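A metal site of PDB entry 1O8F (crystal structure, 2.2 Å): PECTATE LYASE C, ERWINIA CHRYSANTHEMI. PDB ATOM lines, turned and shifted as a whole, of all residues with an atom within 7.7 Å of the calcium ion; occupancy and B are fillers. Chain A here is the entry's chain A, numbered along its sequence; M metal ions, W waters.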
ATOM      1  N   TRP A 106       3.409  24.633 -26.501  1.00  0.00           N
ATOM      2  CA  TRP A 106       2.169  24.695 -25.753  1.00  0.00           C
ATOM      3  C   TRP A 106       1.653  26.122 -25.735  1.00  0.00           C
ATOM      4  O   TRP A 106       2.255  27.001 -25.132  1.00  0.00           O
ATOM      5  CB  TRP A 106       2.414  24.172 -24.337  1.00  0.00           C
ATOM      6  CG  TRP A 106       3.117  22.847 -24.315  1.00  0.00           C
ATOM      7  CD1 TRP A 106       2.954  21.830 -25.221  1.00  0.00           C
ATOM      8  CD2 TRP A 106       4.069  22.371 -23.358  1.00  0.00           C
ATOM      9  NE1 TRP A 106       3.733  20.751 -24.869  1.00  0.00           N
ATOM     10  CE2 TRP A 106       4.430  21.054 -23.730  1.00  0.00           C
ATOM     11  CE3 TRP A 106       4.659  22.934 -22.214  1.00  0.00           C
ATOM     12  CZ2 TRP A 106       5.350  20.283 -23.007  1.00  0.00           C
ATOM     13  CZ3 TRP A 106       5.572  22.161 -21.484  1.00  0.00           C
ATOM     14  CH2 TRP A 106       5.907  20.852 -21.892  1.00  0.00           C
ATOM     15  N   GLY A 126       5.334  11.632 -21.608  1.00  0.00           N
ATOM     16  CA  GLY A 126       3.991  11.248 -21.971  1.00  0.00           C
ATOM     17  C   GLY A 126       3.086  11.208 -20.752  1.00  0.00           C
ATOM     18  O   GLY A 126       1.918  11.584 -20.842  1.00  0.00           O
ATOM     19  N   LYS A 128       3.237  13.133 -18.235  1.00  0.00           N
ATOM     20  CA  LYS A 128       3.071  14.460 -17.674  1.00  0.00           C
ATOM     21  C   LYS A 128       2.701  15.507 -18.722  1.00  0.00           C
ATOM     22  O   LYS A 128       3.145  16.652 -18.669  1.00  0.00           O
ATOM     23  CB  LYS A 128       4.311  14.873 -16.862  1.00  0.00           C
ATOM     24  CG  LYS A 128       4.574  13.993 -15.638  1.00  0.00           C
ATOM     25  CD  LYS A 128       5.816  14.401 -14.896  1.00  0.00           C
ATOM     26  CE  LYS A 128       6.301  13.317 -13.948  1.00  0.00           C
ATOM     27  NZ  LYS A 128       6.999  12.219 -14.654  1.00  0.00           N
ATOM     28  N   ASP A 129       1.862  15.087 -19.664  1.00  0.00           N
ATOM     29  CA  ASP A 129       1.333  15.947 -20.724  1.00  0.00           C
ATOM     30  C   ASP A 129       2.360  16.450 -21.712  1.00  0.00           C
ATOM     31  O   ASP A 129       2.320  17.613 -22.129  1.00  0.00           O
ATOM     32  CB  ASP A 129       0.549  17.119 -20.119  1.00  0.00           C
ATOM     33  CG  ASP A 129      -0.741  17.418 -20.873  1.00  0.00           C
ATOM     34  OD1 ASP A 129      -1.212  16.536 -21.635  1.00  0.00           O
ATOM     35  OD2 ASP A 129      -1.303  18.515 -20.703  1.00  0.00           O
ATOM     36  N   GLY A 130       3.241  15.560 -22.152  1.00  0.00           N
ATOM     37  CA  GLY A 130       4.240  15.967 -23.112  1.00  0.00           C
ATOM     38  C   GLY A 130       3.715  16.058 -24.532  1.00  0.00           C
ATOM     39  O   GLY A 130       4.240  15.394 -25.410  1.00  0.00           O
ATOM     40  N   ASP A 131       2.735  16.923 -24.760  1.00  0.00           N
ATOM     41  CA  ASP A 131       2.154  17.130 -26.083  1.00  0.00           C
ATOM     42  C   ASP A 131       3.123  17.773 -27.056  1.00  0.00           C
ATOM     43  O   ASP A 131       4.000  18.543 -26.650  1.00  0.00           O
ATOM     44  CB  ASP A 131       0.927  18.020 -25.987  1.00  0.00           C
ATOM     45  CG  ASP A 131      -0.207  17.364 -25.245  1.00  0.00           C
ATOM     46  OD1 ASP A 131      -0.455  16.154 -25.472  1.00  0.00           O
ATOM     47  OD2 ASP A 131      -0.858  18.054 -24.451  1.00  0.00           O
ATOM     48  N   MET A 132       2.942  17.498 -28.345  1.00  0.00           N
ATOM     49  CA  MET A 132       3.804  18.068 -29.387  1.00  0.00           C
ATOM     50  C   MET A 132       3.325  19.477 -29.635  1.00  0.00           C
ATOM     51  O   MET A 132       4.129  20.399 -29.747  1.00  0.00           O
ATOM     52  CB  MET A 132       3.747  17.236 -30.672  1.00  0.00           C
ATOM     53  CG  MET A 132       4.117  15.794 -30.410  1.00  0.00           C
ATOM     54  SD  MET A 132       4.550  14.848 -31.844  1.00  0.00           S
ATOM     55  CE  MET A 132       3.557  13.425 -31.600  1.00  0.00           C
ATOM     56  N   ILE A 133       2.017  19.640 -29.755  1.00  0.00           N
ATOM     57  CA  ILE A 133       1.392  20.941 -29.922  1.00  0.00           C
ATOM     58  C   ILE A 133       0.123  20.870 -29.058  1.00  0.00           C
ATOM     59  O   ILE A 133      -0.583  19.860 -29.051  1.00  0.00           O
ATOM     60  CB  ILE A 133       1.005  21.270 -31.391  1.00  0.00           C
ATOM     61  CG1 ILE A 133       2.229  21.209 -32.310  1.00  0.00           C
ATOM     62  CG2 ILE A 133       0.362  22.670 -31.459  1.00  0.00           C
ATOM     63  CD1 ILE A 133       3.068  22.435 -32.338  1.00  0.00           C
ATOM     64  N   ARG A 134      -0.080  21.901 -28.242  1.00  0.00           N
ATOM     65  CA  ARG A 134      -1.267  21.982 -27.395  1.00  0.00           C
ATOM     66  C   ARG A 134      -1.843  23.351 -27.636  1.00  0.00           C
ATOM     67  O   ARG A 134      -1.113  24.338 -27.641  1.00  0.00           O
ATOM     68  CB  ARG A 134      -0.928  21.807 -25.924  1.00  0.00           C
ATOM     69  CG  ARG A 134      -2.145  21.868 -25.041  1.00  0.00           C
ATOM     70  CD  ARG A 134      -1.892  21.141 -23.751  1.00  0.00           C
ATOM     71  NE  ARG A 134      -0.938  21.840 -22.912  1.00  0.00           N
ATOM     72  CZ  ARG A 134       0.145  21.281 -22.406  1.00  0.00           C
ATOM     73  NH1 ARG A 134       0.414  20.004 -22.627  1.00  0.00           N
ATOM     74  NH2 ARG A 134       0.960  22.001 -21.651  1.00  0.00           N
ATOM     75  N   GLU A 166       2.228  11.295 -25.458  1.00  0.00           N
ATOM     76  CA  GLU A 166       1.068  12.134 -25.384  1.00  0.00           C
ATOM     77  C   GLU A 166       0.607  12.404 -26.801  1.00  0.00           C
ATOM     78  O   GLU A 166       0.969  11.671 -27.714  1.00  0.00           O
ATOM     79  CB  GLU A 166       1.350  13.437 -24.632  1.00  0.00           C
ATOM     80  CG  GLU A 166       0.571  13.553 -23.343  1.00  0.00           C
ATOM     81  CD  GLU A 166      -0.914  13.257 -23.518  1.00  0.00           C
ATOM     82  OE1 GLU A 166      -1.618  14.023 -24.207  1.00  0.00           O
ATOM     83  OE2 GLU A 166      -1.373  12.246 -22.964  1.00  0.00           O
ATOM     84  N   SER A 167      -0.084  13.512 -27.005  1.00  0.00           N
ATOM     85  CA  SER A 167      -0.664  13.809 -28.300  1.00  0.00           C
ATOM     86  C   SER A 167       0.112  14.642 -29.285  1.00  0.00           C
ATOM     87  O   SER A 167       1.123  15.255 -28.942  1.00  0.00           O
ATOM     88  CB  SER A 167      -2.022  14.428 -28.059  1.00  0.00           C
ATOM     89  OG  SER A 167      -2.637  13.724 -26.979  1.00  0.00           O
ATOM     90  N   ALA A 168      -0.377  14.667 -30.521  1.00  0.00           N
ATOM     91  CA  ALA A 168       0.255  15.422 -31.582  1.00  0.00           C
ATOM     92  C   ALA A 168      -0.296  16.823 -31.577  1.00  0.00           C
ATOM     93  O   ALA A 168       0.466  17.790 -31.601  1.00  0.00           O
ATOM     94  CB  ALA A 168       0.017  14.748 -32.935  1.00  0.00           C
ATOM     95  N   VAL A 169      -1.626  16.947 -31.546  1.00  0.00           N
ATOM     96  CA  VAL A 169      -2.266  18.249 -31.515  1.00  0.00           C
ATOM     97  C   VAL A 169      -3.516  18.262 -30.650  1.00  0.00           C
ATOM     98  O   VAL A 169      -4.629  18.060 -31.148  1.00  0.00           O
ATOM     99  CB  VAL A 169      -2.669  18.782 -32.936  1.00  0.00           C
ATOM    100  CG1 VAL A 169      -3.095  20.252 -32.861  1.00  0.00           C
ATOM    101  CG2 VAL A 169      -1.535  18.624 -33.913  1.00  0.00           C
ATOM    102  N   ASP A 170      -3.339  18.493 -29.350  1.00  0.00           N
ATOM    103  CA  ASP A 170      -4.478  18.568 -28.430  1.00  0.00           C
ATOM    104  C   ASP A 170      -5.040  19.978 -28.404  1.00  0.00           C
ATOM    105  O   ASP A 170      -4.294  20.950 -28.287  1.00  0.00           O
ATOM    106  CB  ASP A 170      -4.066  18.180 -27.012  1.00  0.00           C
ATOM    107  CG  ASP A 170      -4.228  16.691 -26.747  1.00  0.00           C
ATOM    108  OD1 ASP A 170      -4.789  15.970 -27.601  1.00  0.00           O
ATOM    109  OD2 ASP A 170      -3.832  16.246 -25.645  1.00  0.00           O
ATOM    110  N   ILE A 171      -6.362  20.083 -28.499  1.00  0.00           N
ATOM    111  CA  ILE A 171      -7.054  21.361 -28.481  1.00  0.00           C
ATOM    112  C   ILE A 171      -8.124  21.293 -27.414  1.00  0.00           C
ATOM    113  O   ILE A 171      -8.905  20.352 -27.385  1.00  0.00           O
ATOM    114  CB  ILE A 171      -7.764  21.641 -29.849  1.00  0.00           C
ATOM    115  CG1 ILE A 171      -6.744  21.737 -30.984  1.00  0.00           C
ATOM    116  CG2 ILE A 171      -8.620  22.892 -29.742  1.00  0.00           C
ATOM    117  CD1 ILE A 171      -7.378  21.721 -32.370  1.00  0.00           C
ATOM    118  N   LYS A 172      -8.153  22.293 -26.540  1.00  0.00           N
ATOM    119  CA  LYS A 172      -9.149  22.341 -25.479  1.00  0.00           C
ATOM    120  C   LYS A 172      -9.487  23.766 -25.108  1.00  0.00           C
ATOM    121  O   LYS A 172      -8.909  24.730 -25.648  1.00  0.00           O
ATOM    122  CB  LYS A 172      -8.679  21.571 -24.237  1.00  0.00           C
ATOM    123  CG  LYS A 172      -7.288  21.894 -23.790  1.00  0.00           C
ATOM    124  CD  LYS A 172      -7.057  21.388 -22.368  1.00  0.00           C
ATOM    125  CE  LYS A 172      -5.588  21.466 -21.992  1.00  0.00           C
ATOM    126  NZ  LYS A 172      -5.339  21.286 -20.524  1.00  0.00           N
ATOM    127  N   LYS A 190      -2.423   8.722 -29.769  1.00  0.00           N
ATOM    128  CA  LYS A 190      -3.525   9.644 -29.516  1.00  0.00           C
ATOM    129  C   LYS A 190      -3.234  10.929 -30.244  1.00  0.00           C
ATOM    130  O   LYS A 190      -2.536  11.796 -29.738  1.00  0.00           O
ATOM    131  CB  LYS A 190      -3.655   9.896 -28.021  1.00  0.00           C
ATOM    132  CG  LYS A 190      -3.744   8.606 -27.201  1.00  0.00           C
ATOM    133  CD  LYS A 190      -3.583   8.878 -25.734  1.00  0.00           C
ATOM    134  CE  LYS A 190      -2.292   9.624 -25.450  1.00  0.00           C
ATOM    135  NZ  LYS A 190      -2.144   9.889 -23.998  1.00  0.00           N
ATOM    136  N   LEU A 193      -7.134  15.833 -29.196  1.00  0.00           N
ATOM    137  CA  LEU A 193      -8.417  16.124 -28.602  1.00  0.00           C
ATOM    138  C   LEU A 193      -8.967  17.371 -29.238  1.00  0.00           C
ATOM    139  O   LEU A 193      -8.240  18.139 -29.865  1.00  0.00           O
ATOM    140  CB  LEU A 193      -8.264  16.396 -27.086  1.00  0.00           C
ATOM    141  CG  LEU A 193      -7.844  15.226 -26.197  1.00  0.00           C
ATOM    142  CD1 LEU A 193      -7.648  15.671 -24.786  1.00  0.00           C
ATOM    143  CD2 LEU A 193      -8.909  14.158 -26.266  1.00  0.00           C
ATOM    144  N   ARG A 218      -8.346   9.282 -32.234  1.00  0.00           N
ATOM    145  CA  ARG A 218      -8.556  10.712 -32.023  1.00  0.00           C
ATOM    146  C   ARG A 218      -8.161  11.632 -33.189  1.00  0.00           C
ATOM    147  O   ARG A 218      -7.264  12.460 -33.071  1.00  0.00           O
ATOM    148  CB  ARG A 218      -7.829  11.147 -30.759  1.00  0.00           C
ATOM    149  CG  ARG A 218      -8.180  10.325 -29.564  1.00  0.00           C
ATOM    150  CD  ARG A 218      -7.583  10.910 -28.322  1.00  0.00           C
ATOM    151  NE  ARG A 218      -7.842  10.067 -27.172  1.00  0.00           N
ATOM    152  CZ  ARG A 218      -7.408  10.323 -25.945  1.00  0.00           C
ATOM    153  NH1 ARG A 218      -6.678  11.409 -25.695  1.00  0.00           N
ATOM    154  NH2 ARG A 218      -7.747   9.509 -24.949  1.00  0.00           N
HETATM  155 CA    CA M   1      -2.280  16.358 -23.808  1.00  0.00          CA
HETATM  156  O   HOH W   1      -4.181  15.212 -22.787  1.00  0.00           O
HETATM  157  O   HOH W   2      -3.490  18.283 -23.251  1.00  0.00           O
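The calcium ion is bound by the side-chain carboxylate (OD2) of Asp 131 (2.3 Å), water W2 (2.3 Å), the side-chain carboxylate (OD2) of Asp 170 (2.4 Å), the side-chain carboxylate (OD1) of Asp 129 (2.4 Å), water W1 (2.4 Å), the side-chain carboxylate (OE1) of Glu 166 (2.5 Å) and the side-chain carboxylate (OD1) of Asp 131 (2.5 Å).
OD1 of Asp 131 sits close to N of Ser 167, 3.1 Å away.
OD2 of Asp 131 lies close to NH1 of Arg 134 (3.0 Å).
The indole nitrogen of Trp 106 is in hydrogen-bond range of the backbone carbonyl oxygen of Asp 131 (2.8 Å).
OD1 of Asp 170 is in hydrogen-bond range of OG of Ser 167 (3.2 Å).
The side-chain carboxylate of Asp 170 is in hydrogen-bond range of the backbone NH of Leu 193, 2.8 Å away.
The backbone carbonyl oxygen (O) of Ile 133 is in hydrogen-bond range of the backbone NH (N) of Asp 170, 3.1 Å away.
OD2 of Asp 129 lies within salt-bridge range of NH1 of Arg 134, at 3.0 Å.
The side-chain carboxylate (OE1) of Glu 166 lies close to the side-chain hydroxyl (OG) of Ser 167, at 3.0 Å.
Of the 19 residues printed, 4 come within 4 Å of the calcium ion.
The nearest printed residue that does not touch the calcium ion is Ser 167 (4.1 Å).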
